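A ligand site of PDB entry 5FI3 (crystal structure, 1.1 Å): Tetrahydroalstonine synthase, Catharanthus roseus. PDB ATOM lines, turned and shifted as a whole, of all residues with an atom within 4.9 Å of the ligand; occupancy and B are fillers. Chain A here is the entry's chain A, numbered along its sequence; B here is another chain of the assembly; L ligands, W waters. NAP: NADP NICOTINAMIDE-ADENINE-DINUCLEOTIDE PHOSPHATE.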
ATOM      1  N   CYS A  55      25.295 -15.199   0.775  1.00  0.00           N
ATOM      2  CA  CYS A  55      24.236 -16.096   0.342  1.00  0.00           C
ATOM      3  C   CYS A  55      22.977 -15.320   0.062  1.00  0.00           C
ATOM      4  O   CYS A  55      22.913 -14.092   0.284  1.00  0.00           O
ATOM      5  CB  CYS A  55      23.993 -17.174   1.412  1.00  0.00           C
ATOM      6  SG  CYS A  55      23.217 -16.519   2.903  1.00  0.00           S
ATOM      7  N   GLN A  56      21.965 -16.034  -0.412  1.00  0.00           N
ATOM      8  CA  GLN A  56      20.700 -15.425  -0.766  1.00  0.00           C
ATOM      9  C   GLN A  56      20.117 -14.622   0.377  1.00  0.00           C
ATOM     10  O   GLN A  56      19.523 -13.590   0.149  1.00  0.00           O
ATOM     11  CB  GLN A  56      19.719 -16.489  -1.256  1.00  0.00           C
ATOM     12  CG  GLN A  56      18.468 -15.964  -1.899  1.00  0.00           C
ATOM     13  CD  GLN A  56      18.772 -15.156  -3.137  1.00  0.00           C
ATOM     14  OE1 GLN A  56      18.565 -13.959  -3.157  1.00  0.00           O
ATOM     15  NE2 GLN A  56      19.304 -15.805  -4.154  1.00  0.00           N
ATOM     16  N   TYR A  57      20.239 -15.099   1.612  1.00  0.00           N
ATOM     17  CA  TYR A  57      19.718 -14.389   2.759  1.00  0.00           C
ATOM     18  C   TYR A  57      20.268 -12.977   2.852  1.00  0.00           C
ATOM     19  O   TYR A  57      19.554 -12.029   3.171  1.00  0.00           O
ATOM     20  CB  TYR A  57      20.005 -15.134   4.053  1.00  0.00           C
ATOM     21  CG  TYR A  57      19.442 -14.479   5.281  1.00  0.00           C
ATOM     22  CD1 TYR A  57      18.104 -14.666   5.643  1.00  0.00           C
ATOM     23  CD2 TYR A  57      20.237 -13.697   6.100  1.00  0.00           C
ATOM     24  CE1 TYR A  57      17.581 -14.094   6.778  1.00  0.00           C
ATOM     25  CE2 TYR A  57      19.710 -13.102   7.242  1.00  0.00           C
ATOM     26  CZ  TYR A  57      18.382 -13.323   7.575  1.00  0.00           C
ATOM     27  OH  TYR A  57      17.857 -12.758   8.705  1.00  0.00           O
ATOM     28  N   GLU A  60      18.445 -10.967   0.173  1.00  0.00           N
ATOM     29  CA  GLU A  60      17.064 -10.764   0.634  1.00  0.00           C
ATOM     30  C   GLU A  60      17.009  -9.694   1.712  1.00  0.00           C
ATOM     31  O   GLU A  60      16.192  -8.774   1.627  1.00  0.00           O
ATOM     32  CB  GLU A  60      16.467 -12.065   1.150  1.00  0.00           C
ATOM     33  CG  GLU A  60      16.247 -13.138   0.107  1.00  0.00           C
ATOM     34  CD  GLU A  60      15.969 -14.505   0.715  1.00  0.00           C
ATOM     35  OE1 GLU A  60      16.663 -14.824   1.708  1.00  0.00           O
ATOM     36  OE2 GLU A  60      15.084 -15.247   0.237  1.00  0.00           O
ATOM     37  N   LYS A  65      13.410  -7.885   2.052  1.00  0.00           N
ATOM     38  CA  LYS A  65      12.368  -8.831   1.591  1.00  0.00           C
ATOM     39  C   LYS A  65      11.357  -9.162   2.695  1.00  0.00           C
ATOM     40  O   LYS A  65      10.171  -9.308   2.434  1.00  0.00           O
ATOM     41  CB  LYS A  65      12.979 -10.124   1.097  1.00  0.00           C
ATOM     42  CG  LYS A  65      11.973 -11.206   0.669  1.00  0.00           C
ATOM     43  CD  LYS A  65      12.674 -12.455   0.151  1.00  0.00           C
ATOM     44  CE  LYS A  65      11.693 -13.581  -0.169  1.00  0.00           C
ATOM     45  NZ  LYS A  65      12.393 -14.781  -0.698  1.00  0.00           N
ATOM     46  N   PHE A  66      11.857  -9.291   3.926  1.00  0.00           N
ATOM     47  CA  PHE A  66      11.062  -9.781   5.051  1.00  0.00           C
ATOM     48  C   PHE A  66      10.482  -8.659   5.911  1.00  0.00           C
ATOM     49  O   PHE A  66       9.696  -8.928   6.818  1.00  0.00           O
ATOM     50  CB  PHE A  66      11.921 -10.709   5.912  1.00  0.00           C
ATOM     51  CG  PHE A  66      12.591 -11.786   5.106  1.00  0.00           C
ATOM     52  CD1 PHE A  66      11.831 -12.684   4.363  1.00  0.00           C
ATOM     53  CD2 PHE A  66      13.980 -11.869   5.044  1.00  0.00           C
ATOM     54  CE1 PHE A  66      12.445 -13.665   3.594  1.00  0.00           C
ATOM     55  CE2 PHE A  66      14.587 -12.841   4.283  1.00  0.00           C
ATOM     56  CZ  PHE A  66      13.820 -13.736   3.554  1.00  0.00           C
ATOM     57  N   CYS A 163      26.341 -21.735   7.631  1.00  0.00           N
ATOM     58  CA  CYS A 163      25.033 -21.226   7.206  1.00  0.00           C
ATOM     59  C   CYS A 163      24.278 -22.403   6.582  1.00  0.00           C
ATOM     60  O   CYS A 163      23.368 -22.964   7.213  1.00  0.00           O
ATOM     61  CB  CYS A 163      25.201 -20.053   6.263  1.00  0.00           C
ATOM     62  SG  CYS A 163      23.661 -19.437   5.550  1.00  0.00           S
ATOM     63  N   THR A 167      22.044 -25.305   8.755  1.00  0.00           N
ATOM     64  CA  THR A 167      20.604 -25.183   8.457  1.00  0.00           C
ATOM     65  C   THR A 167      20.041 -26.491   7.942  1.00  0.00           C
ATOM     66  O   THR A 167      18.891 -26.824   8.257  1.00  0.00           O
ATOM     67  CB  THR A 167      20.379 -24.013   7.517  1.00  0.00           C
ATOM     68  OG1 THR A 167      20.748 -22.792   8.196  1.00  0.00           O
ATOM     69  CG2 THR A 167      18.942 -23.885   7.081  1.00  0.00           C
ATOM     70  N   GLY A 188      15.379 -27.427  -5.054  1.00  0.00           N
ATOM     71  CA  GLY A 188      16.175 -26.252  -5.340  1.00  0.00           C
ATOM     72  C   GLY A 188      17.652 -26.573  -5.127  1.00  0.00           C
ATOM     73  O   GLY A 188      18.115 -26.669  -4.000  1.00  0.00           O
ATOM     74  N   LEU A 189      18.369 -26.761  -6.234  1.00  0.00           N
ATOM     75  CA  LEU A 189      19.802 -27.101  -6.155  1.00  0.00           C
ATOM     76  C   LEU A 189      20.606 -25.815  -6.192  1.00  0.00           C
ATOM     77  O   LEU A 189      21.272 -25.472  -7.187  1.00  0.00           O
ATOM     78  CB  LEU A 189      20.177 -28.067  -7.261  1.00  0.00           C
ATOM     79  CG  LEU A 189      21.641 -28.557  -7.241  1.00  0.00           C
ATOM     80  CD1 LEU A 189      21.996 -29.205  -5.914  1.00  0.00           C
ATOM     81  CD2 LEU A 189      21.885 -29.548  -8.361  1.00  0.00           C
ATOM     82  N   GLY A 190      20.558 -25.086  -5.098  1.00  0.00           N
ATOM     83  CA  GLY A 190      21.257 -23.811  -4.967  1.00  0.00           C
ATOM     84  C   GLY A 190      22.241 -23.850  -3.831  1.00  0.00           C
ATOM     85  O   GLY A 190      22.872 -24.866  -3.509  1.00  0.00           O
ATOM     86  N   GLY A 191      22.401 -22.699  -3.207  1.00  0.00           N
ATOM     87  CA  GLY A 191      23.422 -22.560  -2.169  1.00  0.00           C
ATOM     88  C   GLY A 191      23.183 -23.523  -1.030  1.00  0.00           C
ATOM     89  O   GLY A 191      24.046 -24.321  -0.659  1.00  0.00           O
ATOM     90  N   LEU A 192      21.992 -23.458  -0.465  1.00  0.00           N
ATOM     91  CA  LEU A 192      21.643 -24.362   0.600  1.00  0.00           C
ATOM     92  C   LEU A 192      21.475 -25.822   0.123  1.00  0.00           C
ATOM     93  O   LEU A 192      21.955 -26.774   0.750  1.00  0.00           O
ATOM     94  CB  LEU A 192      20.379 -23.800   1.247  1.00  0.00           C
ATOM     95  CG  LEU A 192      19.765 -24.647   2.321  1.00  0.00           C
ATOM     96  CD1 LEU A 192      20.698 -24.958   3.463  1.00  0.00           C
ATOM     97  CD2 LEU A 192      18.524 -23.945   2.825  1.00  0.00           C
ATOM     98  N   GLY A 193      20.810 -25.975  -1.012  1.00  0.00           N
ATOM     99  CA  GLY A 193      20.503 -27.293  -1.522  1.00  0.00           C
ATOM    100  C   GLY A 193      21.715 -28.150  -1.832  1.00  0.00           C
ATOM    101  O   GLY A 193      21.705 -29.355  -1.570  1.00  0.00           O
ATOM    102  N   ILE A 210      14.937 -32.049  -7.061  1.00  0.00           N
ATOM    103  CA  ILE A 210      13.753 -31.439  -7.656  1.00  0.00           C
ATOM    104  C   ILE A 210      14.156 -30.037  -8.020  1.00  0.00           C
ATOM    105  O   ILE A 210      14.544 -29.257  -7.146  1.00  0.00           O
ATOM    106  CB  ILE A 210      12.576 -31.465  -6.685  1.00  0.00           C
ATOM    107  CG1 ILE A 210      12.272 -32.906  -6.218  1.00  0.00           C
ATOM    108  CG2 ILE A 210      11.364 -30.854  -7.333  1.00  0.00           C
ATOM    109  CD1 ILE A 210      12.290 -33.119  -4.743  1.00  0.00           C
ATOM    110  N   SER A 211      14.091 -29.692  -9.297  1.00  0.00           N
ATOM    111  CA  SER A 211      14.621 -28.425  -9.793  1.00  0.00           C
ATOM    112  C   SER A 211      13.629 -27.762 -10.737  1.00  0.00           C
ATOM    113  O   SER A 211      12.685 -28.390 -11.228  1.00  0.00           O
ATOM    114  CB  SER A 211      15.956 -28.693 -10.479  1.00  0.00           C
ATOM    115  OG  SER A 211      16.645 -27.521 -10.863  1.00  0.00           O
ATOM    116  N   SER A 212      13.853 -26.478 -11.001  1.00  0.00           N
ATOM    117  CA  SER A 212      12.912 -25.685 -11.782  1.00  0.00           C
ATOM    118  C   SER A 212      13.067 -25.832 -13.287  1.00  0.00           C
ATOM    119  O   SER A 212      12.260 -25.295 -14.027  1.00  0.00           O
ATOM    120  CB  SER A 212      13.030 -24.215 -11.391  1.00  0.00           C
ATOM    121  OG  SER A 212      14.322 -23.683 -11.598  1.00  0.00           O
ATOM    122  N   SER A 213      14.095 -26.548 -13.736  1.00  0.00           N
ATOM    123  CA  SER A 213      14.309 -26.751 -15.167  1.00  0.00           C
ATOM    124  C   SER A 213      15.326 -27.883 -15.312  1.00  0.00           C
ATOM    125  O   SER A 213      15.888 -28.364 -14.330  1.00  0.00           O
ATOM    126  CB  SER A 213      14.828 -25.484 -15.819  1.00  0.00           C
ATOM    127  OG  SER A 213      16.169 -25.265 -15.451  1.00  0.00           O
ATOM    128  N   LYS A 216      20.275 -27.702 -14.517  1.00  0.00           N
ATOM    129  CA  LYS A 216      21.258 -28.269 -13.572  1.00  0.00           C
ATOM    130  C   LYS A 216      21.339 -29.777 -13.582  1.00  0.00           C
ATOM    131  O   LYS A 216      21.983 -30.369 -12.727  1.00  0.00           O
ATOM    132  CB  LYS A 216      20.998 -27.753 -12.157  1.00  0.00           C
ATOM    133  CG  LYS A 216      21.271 -26.288 -11.982  1.00  0.00           C
ATOM    134  CD  LYS A 216      20.856 -25.782 -10.636  1.00  0.00           C
ATOM    135  CE  LYS A 216      21.241 -24.339 -10.434  1.00  0.00           C
ATOM    136  NZ  LYS A 216      20.560 -23.765  -9.253  1.00  0.00           N
ATOM    137  N   THR A 251      14.381 -25.903  -0.179  1.00  0.00           N
ATOM    138  CA  THR A 251      15.191 -24.689  -0.054  1.00  0.00           C
ATOM    139  C   THR A 251      14.654 -23.524  -0.846  1.00  0.00           C
ATOM    140  O   THR A 251      15.275 -22.466  -0.860  1.00  0.00           O
ATOM    141  CB  THR A 251      16.642 -24.956  -0.500  1.00  0.00           C
ATOM    142  OG1 THR A 251      16.743 -24.975  -1.927  1.00  0.00           O
ATOM    143  CG2 THR A 251      17.201 -26.232   0.110  1.00  0.00           C
ATOM    144  N   ILE A 252      13.521 -23.695  -1.514  1.00  0.00           N
ATOM    145  CA  ILE A 252      13.121 -22.719  -2.506  1.00  0.00           C
ATOM    146  C   ILE A 252      12.722 -21.397  -1.860  1.00  0.00           C
ATOM    147  O   ILE A 252      11.876 -21.378  -0.965  1.00  0.00           O
ATOM    148  CB  ILE A 252      11.976 -23.285  -3.359  1.00  0.00           C
ATOM    149  CG1 ILE A 252      12.470 -24.487  -4.186  1.00  0.00           C
ATOM    150  CG2 ILE A 252      11.358 -22.200  -4.232  1.00  0.00           C
ATOM    151  CD1 ILE A 252      11.345 -25.313  -4.771  1.00  0.00           C
ATOM    152  N   PRO A 253      13.281 -20.281  -2.349  1.00  0.00           N
ATOM    153  CA  PRO A 253      13.015 -18.996  -1.728  1.00  0.00           C
ATOM    154  C   PRO A 253      11.853 -18.239  -2.330  1.00  0.00           C
ATOM    155  O   PRO A 253      11.385 -17.291  -1.725  1.00  0.00           O
ATOM    156  CB  PRO A 253      14.321 -18.208  -2.035  1.00  0.00           C
ATOM    157  CG  PRO A 253      14.818 -18.761  -3.311  1.00  0.00           C
ATOM    158  CD  PRO A 253      14.492 -20.220  -3.198  1.00  0.00           C
ATOM    159  N   GLY A 254      11.427 -18.617  -3.535  1.00  0.00           N
ATOM    160  CA  GLY A 254      10.359 -17.971  -4.251  1.00  0.00           C
ATOM    161  C   GLY A 254       9.021 -18.674  -4.096  1.00  0.00           C
ATOM    162  O   GLY A 254       8.945 -19.761  -3.532  1.00  0.00           O
ATOM    163  N   ASN A 255       7.967 -18.020  -4.570  1.00  0.00           N
ATOM    164  CA  ASN A 255       6.632 -18.565  -4.427  1.00  0.00           C
ATOM    165  C   ASN A 255       6.525 -19.919  -5.087  1.00  0.00           C
ATOM    166  O   ASN A 255       6.909 -20.086  -6.245  1.00  0.00           O
ATOM    167  CB  ASN A 255       5.613 -17.622  -5.050  1.00  0.00           C
ATOM    168  CG  ASN A 255       5.617 -16.248  -4.419  1.00  0.00           C
ATOM    169  OD1 ASN A 255       6.023 -16.067  -3.261  1.00  0.00           O
ATOM    170  ND2 ASN A 255       5.155 -15.277  -5.172  1.00  0.00           N
ATOM    171  N   LEU A 274      12.776 -24.764   4.515  1.00  0.00           N
ATOM    172  CA  LEU A 274      13.891 -23.932   4.937  1.00  0.00           C
ATOM    173  C   LEU A 274      13.839 -22.643   4.235  1.00  0.00           C
ATOM    174  O   LEU A 274      14.222 -21.605   4.789  1.00  0.00           O
ATOM    175  CB  LEU A 274      15.250 -24.594   4.627  1.00  0.00           C
ATOM    176  CG  LEU A 274      15.477 -25.942   5.264  1.00  0.00           C
ATOM    177  CD1 LEU A 274      16.835 -26.517   4.883  1.00  0.00           C
ATOM    178  CD2 LEU A 274      15.367 -25.825   6.771  1.00  0.00           C
ATOM    179  N   GLY A 275      13.391 -22.686   2.994  1.00  0.00           N
ATOM    180  CA  GLY A 275      13.365 -21.449   2.263  1.00  0.00           C
ATOM    181  C   GLY A 275      12.182 -20.611   2.662  1.00  0.00           C
ATOM    182  O   GLY A 275      11.197 -21.136   3.216  1.00  0.00           O
ATOM    183  N   ALA A 276      12.237 -19.317   2.359  1.00  0.00           N
ATOM    184  CA  ALA A 276      11.263 -18.346   2.853  1.00  0.00           C
ATOM    185  C   ALA A 276      10.580 -17.472   1.775  1.00  0.00           C
ATOM    186  O   ALA A 276      11.035 -16.340   1.566  1.00  0.00           O
ATOM    187  CB  ALA A 276      11.987 -17.449   3.868  1.00  0.00           C
ATOM    188  N   SER A 298      12.367 -25.019   9.832  1.00  0.00           N
ATOM    189  CA  SER A 298      13.541 -25.018  10.699  1.00  0.00           C
ATOM    190  C   SER A 298      14.368 -23.793  10.405  1.00  0.00           C
ATOM    191  O   SER A 298      14.407 -23.346   9.269  1.00  0.00           O
ATOM    192  CB  SER A 298      14.357 -26.279  10.437  1.00  0.00           C
ATOM    193  OG  SER A 298      15.414 -26.452  11.349  1.00  0.00           O
ATOM    194  N   THR A 299      15.031 -23.266  11.434  1.00  0.00           N
ATOM    195  CA  THR A 299      15.967 -22.169  11.248  1.00  0.00           C
ATOM    196  C   THR A 299      17.285 -22.477  11.944  1.00  0.00           C
ATOM    197  O   THR A 299      17.322 -22.910  13.081  1.00  0.00           O
ATOM    198  CB  THR A 299      15.398 -20.838  11.761  1.00  0.00           C
ATOM    199  OG1 THR A 299      15.053 -20.948  13.134  1.00  0.00           O
ATOM    200  CG2 THR A 299      14.200 -20.398  10.973  1.00  0.00           C
ATOM    201  N   ALA A 300      18.381 -22.226  11.220  1.00  0.00           N
ATOM    202  CA  ALA A 300      19.711 -22.299  11.761  1.00  0.00           C
ATOM    203  C   ALA A 300      19.914 -23.605  12.535  1.00  0.00           C
ATOM    204  O   ALA A 300      19.497 -24.675  12.095  1.00  0.00           O
ATOM    205  CB  ALA A 300      20.016 -21.023  12.561  1.00  0.00           C
ATOM    206  N   LEU A 337      23.200 -13.118  -7.432  1.00  0.00           N
ATOM    207  CA  LEU A 337      22.278 -13.877  -6.562  1.00  0.00           C
ATOM    208  C   LEU A 337      20.807 -13.775  -6.969  1.00  0.00           C
ATOM    209  O   LEU A 337      20.035 -14.688  -6.713  1.00  0.00           O
ATOM    210  CB  LEU A 337      22.444 -13.519  -5.100  1.00  0.00           C
ATOM    211  CG  LEU A 337      23.745 -14.035  -4.487  1.00  0.00           C
ATOM    212  CD1 LEU A 337      23.913 -13.451  -3.085  1.00  0.00           C
ATOM    213  CD2 LEU A 337      23.755 -15.547  -4.400  1.00  0.00           C
ATOM    214  N   SER A 340      20.442 -16.734  -8.828  1.00  0.00           N
ATOM    215  CA  SER A 340      21.219 -17.811  -8.316  1.00  0.00           C
ATOM    216  C   SER A 340      22.380 -18.193  -9.262  1.00  0.00           C
ATOM    217  O   SER A 340      22.688 -19.362  -9.460  1.00  0.00           O
ATOM    218  CB  SER A 340      20.245 -18.993  -8.110  1.00  0.00           C
ATOM    219  OG  SER A 340      20.870 -20.021  -7.435  1.00  0.00           O
ATOM    220  N   TYR A 344      28.591 -22.781  -6.076  1.00  0.00           N
ATOM    221  CA  TYR A 344      27.212 -22.552  -5.645  1.00  0.00           C
ATOM    222  C   TYR A 344      27.070 -21.513  -4.545  1.00  0.00           C
ATOM    223  O   TYR A 344      25.941 -21.185  -4.188  1.00  0.00           O
ATOM    224  CB  TYR A 344      26.555 -23.886  -5.211  1.00  0.00           C
ATOM    225  CG  TYR A 344      26.225 -24.781  -6.373  1.00  0.00           C
ATOM    226  CD1 TYR A 344      27.207 -25.549  -6.997  1.00  0.00           C
ATOM    227  CD2 TYR A 344      24.943 -24.813  -6.920  1.00  0.00           C
ATOM    228  CE1 TYR A 344      26.925 -26.298  -8.126  1.00  0.00           C
ATOM    229  CE2 TYR A 344      24.646 -25.550  -8.026  1.00  0.00           C
ATOM    230  CZ  TYR A 344      25.636 -26.296  -8.632  1.00  0.00           C
ATOM    231  OH  TYR A 344      25.286 -27.036  -9.744  1.00  0.00           O
ATOM    232  N   ARG A 345      28.188 -21.017  -3.998  1.00  0.00           N
ATOM    233  CA  ARG A 345      28.190 -19.979  -2.970  1.00  0.00           C
ATOM    234  C   ARG A 345      29.312 -19.018  -3.247  1.00  0.00           C
ATOM    235  O   ARG A 345      30.407 -19.460  -3.583  1.00  0.00           O
ATOM    236  CB  ARG A 345      28.524 -20.573  -1.586  1.00  0.00           C
ATOM    237  CG  ARG A 345      27.613 -21.688  -1.180  1.00  0.00           C
ATOM    238  CD  ARG A 345      26.299 -21.130  -0.668  1.00  0.00           C
ATOM    239  NE  ARG A 345      26.370 -20.631   0.698  1.00  0.00           N
ATOM    240  CZ  ARG A 345      25.345 -20.645   1.544  1.00  0.00           C
ATOM    241  NH1 ARG A 345      24.144 -21.099   1.157  1.00  0.00           N
ATOM    242  NH2 ARG A 345      25.487 -20.211   2.781  1.00  0.00           N
ATOM    243  N   LEU B 289       8.310 -20.977  10.229  1.00  0.00           N
ATOM    244  CA  LEU B 289       9.747 -20.732  10.350  1.00  0.00           C
ATOM    245  C   LEU B 289      10.086 -20.114  11.659  1.00  0.00           C
ATOM    246  O   LEU B 289      11.091 -20.506  12.244  1.00  0.00           O
ATOM    247  CB  LEU B 289      10.257 -19.855   9.219  1.00  0.00           C
ATOM    248  CG  LEU B 289      10.455 -20.559   7.892  1.00  0.00           C
ATOM    249  CD1 LEU B 289      10.484 -19.502   6.807  1.00  0.00           C
ATOM    250  CD2 LEU B 289      11.743 -21.400   7.885  1.00  0.00           C
HETATM  251  PA  NAP L   1      19.858 -19.836  -3.708  1.00  0.00           P
HETATM  252  O1A NAP L   1      19.350 -18.646  -4.478  1.00  0.00           O
HETATM  253  O2A NAP L   1      21.348 -20.114  -3.694  1.00  0.00           O
HETATM  254  O5B NAP L   1      19.198 -21.209  -4.139  1.00  0.00           O
HETATM  255  C5B NAP L   1      17.778 -21.334  -4.186  1.00  0.00           C
HETATM  256  C4B NAP L   1      17.451 -22.358  -5.259  1.00  0.00           C
HETATM  257  O4B NAP L   1      16.008 -22.461  -5.275  1.00  0.00           O
HETATM  258  C3B NAP L   1      17.815 -21.915  -6.666  1.00  0.00           C
HETATM  259  O3B NAP L   1      19.131 -22.258  -7.065  1.00  0.00           O
HETATM  260  C2B NAP L   1      16.758 -22.607  -7.502  1.00  0.00           C
HETATM  261  O2B NAP L   1      17.126 -23.988  -7.665  1.00  0.00           O
HETATM  262  C1B NAP L   1      15.525 -22.563  -6.606  1.00  0.00           C
HETATM  263  N9A NAP L   1      14.623 -21.454  -6.865  1.00  0.00           N
HETATM  264  C8A NAP L   1      14.864 -20.117  -6.719  1.00  0.00           C
HETATM  265  N7A NAP L   1      13.814 -19.359  -6.951  1.00  0.00           N
HETATM  266  C5A NAP L   1      12.828 -20.274  -7.279  1.00  0.00           C
HETATM  267  C6A NAP L   1      11.467 -20.112  -7.592  1.00  0.00           C
HETATM  268  N6A NAP L   1      10.877 -18.920  -7.675  1.00  0.00           N
HETATM  269  N1A NAP L   1      10.755 -21.243  -7.824  1.00  0.00           N
HETATM  270  C2A NAP L   1      11.362 -22.427  -7.773  1.00  0.00           C
HETATM  271  N3A NAP L   1      12.633 -22.696  -7.489  1.00  0.00           N
HETATM  272  C4A NAP L   1      13.316 -21.566  -7.245  1.00  0.00           C
HETATM  273  O3  NAP L   1      19.335 -19.581  -2.199  1.00  0.00           O
HETATM  274  PN  NAP L   1      19.810 -20.341  -0.868  1.00  0.00           P
HETATM  275  O1N NAP L   1      19.814 -21.802  -1.142  1.00  0.00           O
HETATM  276  O2N NAP L   1      21.035 -19.706  -0.369  1.00  0.00           O
HETATM  277  O5D NAP L   1      18.681 -19.907   0.148  1.00  0.00           O
HETATM  278  C5D NAP L   1      17.360 -20.386  -0.096  1.00  0.00           C
HETATM  279  C4D NAP L   1      16.436 -19.841   0.945  1.00  0.00           C
HETATM  280  O4D NAP L   1      16.809 -20.338   2.230  1.00  0.00           O
HETATM  281  C3D NAP L   1      16.372 -18.325   1.067  1.00  0.00           C
HETATM  282  O3D NAP L   1      14.987 -17.951   1.137  1.00  0.00           O
HETATM  283  C2D NAP L   1      17.120 -18.042   2.367  1.00  0.00           C
HETATM  284  O2D NAP L   1      16.668 -16.898   3.070  1.00  0.00           O
HETATM  285  C1D NAP L   1      16.720 -19.270   3.148  1.00  0.00           C
HETATM  286  N1N NAP L   1      17.601 -19.559   4.318  1.00  0.00           N
HETATM  287  C2N NAP L   1      16.969 -20.031   5.403  1.00  0.00           C
HETATM  288  C3N NAP L   1      17.695 -20.411   6.503  1.00  0.00           C
HETATM  289  C7N NAP L   1      17.031 -21.103   7.637  1.00  0.00           C
HETATM  290  O7N NAP L   1      17.596 -21.130   8.722  1.00  0.00           O
HETATM  291  N7N NAP L   1      15.809 -21.627   7.439  1.00  0.00           N
HETATM  292  C4N NAP L   1      19.087 -20.242   6.493  1.00  0.00           C
HETATM  293  C5N NAP L   1      19.712 -19.767   5.359  1.00  0.00           C
HETATM  294  C6N NAP L   1      18.950 -19.453   4.255  1.00  0.00           C
HETATM  295  P2B NAP L   1      16.999 -24.680  -9.116  1.00  0.00           P
HETATM  296  O1X NAP L   1      17.495 -26.067  -8.862  1.00  0.00           O
HETATM  297  O2X NAP L   1      17.856 -23.868 -10.023  1.00  0.00           O
HETATM  298  O3X NAP L   1      15.552 -24.612  -9.524  1.00  0.00           O
HETATM  299  O   HOH W   1      16.598 -17.790   8.137  1.00  0.00           O
HETATM  300  O   HOH W   2      13.531 -25.365  -7.769  1.00  0.00           O
HETATM  301  O   HOH W   3      20.842 -18.308   1.961  1.00  0.00           O
HETATM  302  O   HOH W   4      22.812 -18.770  -5.507  1.00  0.00           O
HETATM  303  O   HOH W   5      23.079 -18.623  -1.291  1.00  0.00           O
HETATM  304  O   HOH W   6       8.058 -21.797  -8.175  1.00  0.00           O
HETATM  305  O   HOH W   7      17.139 -18.020  -5.957  1.00  0.00           O
HETATM  306  O   HOH W   8      11.431 -16.031  -7.202  1.00  0.00           O
HETATM  307  O   HOH W   9      15.310 -17.127   5.553  1.00  0.00           O
HETATM  308  O   HOH W  10      13.725 -16.688  -6.199  1.00  0.00           O
HETATM  309  O   HOH W  11       9.892 -23.792 -10.448  1.00  0.00           O
HETATM  310  O   HOH W  12      18.362 -24.120 -12.649  1.00  0.00           O
HETATM  311  O   HOH W  13      17.889 -21.271 -10.834  1.00  0.00           O
HETATM  312  O   HOH W  14      18.310 -18.812  10.029  1.00  0.00           O
HETATM  313  O   HOH W  15       8.043 -18.412  -8.218  1.00  0.00           O
HETATM  314  O   HOH W  16      19.322 -24.146  -2.524  1.00  0.00           O
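O2D of the ligand is in hydrogen-bond range of OE1 of Glu 60, at 2.5 Å.
The backbone NH of Ser 212 lies within hydrogen-bond range of an oxygen (O3X) of the ligand (2.9 Å).
The side-chain hydroxyl (OG) of Ser 212 lies within hydrogen-bond range of an oxygen (O3X) of the ligand.
The side-chain hydroxyl (OG) of Ser 211 sits at hydrogen-bond distance from an oxygen (O1X) of the ligand (2.6 Å).
The side-chain amino group (NZ) of Lys 216 lies within salt-bridge range of an oxygen (O2X) of the ligand (2.8 Å).
The backbone NH (N) of Leu 192 lies within hydrogen-bond range of an oxygen (O1N) of the ligand (2.8 Å).
An oxygen (O2A) of the ligand sits at hydrogen-bond distance from the backbone NH (N) of Gly 191.
O7N of the ligand is in hydrogen-bond range of N of Ala 300, at 2.8 Å.
N of Leu 189 is in hydrogen-bond range of O1X of the ligand.
OG of Ser 340 is in hydrogen-bond range of O3B of the ligand.
The side-chain amide nitrogen (NE2) of Gln 56 sits at hydrogen-bond distance from an oxygen (O1A) of the ligand, 2.9 Å away.
N7N of the ligand sits at hydrogen-bond distance from O of Ser 298 (2.9 Å).
A nitrogen (N7N) of the ligand lies within hydrogen-bond range of the backbone carbonyl oxygen (O) of Leu 274.
The backbone NH (N) of Ala 276 lies within hydrogen-bond range of an oxygen (O3D) of the ligand, at 3.3 Å.
An oxygen (O2N) of the ligand is in salt-bridge range of the guanidinium group of Arg 345 (3.7 Å).
The side-chain carboxylate (OE2) of Glu 60 is in salt-bridge range of the side-chain amino group (NZ) of Lys 65 (2.9 Å).
The side-chain amino group (NZ) of Lys 216 lies within hydrogen-bond range of the backbone carbonyl oxygen (O) of Leu 189 (2.8 Å).
The side-chain amide nitrogen (NE2) of Gln 56 is in hydrogen-bond range of the backbone carbonyl oxygen (O) of Leu 337, at 2.9 Å.
The backbone carbonyl oxygen (O) of Gly 188 is in hydrogen-bond range of the side-chain hydroxyl (OG1) of Thr 251 (3.0 Å).
NZ of Lys 65 lies within hydrogen-bond range of O of Ala 276.
O of Ile 210 lies within hydrogen-bond range of N of Gly 188 (2.9 Å).
OG1 of Thr 167 lies within hydrogen-bond range of O of Cys 163 (2.8 Å).
The guanidinium group (NH2) of Arg 345 sits close to the side-chain sulfur (SG) of Cys 163, 3.4 Å away.
CD1 of Tyr 57 touches O2D of the ligand, 3.7 Å away.
Cys 163 touches the ligand (SG to C5N, 3.97 Å).
Thr 167 touches the ligand.
Gly 188 touches the ligand.
Gly 190 touches the ligand (CA to O3B, 3.4 Å).
Thr 251 touches the ligand.
Ile 252 touches the ligand.
Pro 253 touches the ligand (CB to O3D, 3.3 Å).
CA of Gly 254 touches N6A of the ligand, 3.6 Å away.
Gly 275 touches the ligand.
Thr 299 touches the ligand (CA to O7N, 3.2 Å).
Hydrophobic or aromatic side chains that line the ligand: Tyr 57, Leu 189, Leu 192, Ile 252 and Pro 253.
Of the 35 residues printed, 25 come within 4 Å of the ligand.
Water W5 bridges an oxygen (O2N) of the ligand (2.5 Å) and the backbone NH of Gln 56 (3.0 Å).
Water W4 lies within hydrogen-bond range of an oxygen (O2A) of the ligand (2.7 Å) and the side-chain hydroxyl of Ser 340 (3.0 Å).
Water W3 lies within hydrogen-bond range of an oxygen (O2N) of the ligand (2.7 Å), the backbone NH of Tyr 57 (3.3 Å) and the backbone NH of Gln 56 (3.5 Å).
Water W6 bridges N1A of the ligand (2.8 Å) and O of Asn 255 (2.8 Å).
Water W2 bridges O3X of the ligand (2.8 Å) and N of Ser 212 (3.4 Å).
Water W15 bridges O of Asn 255 and N6A of the ligand.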
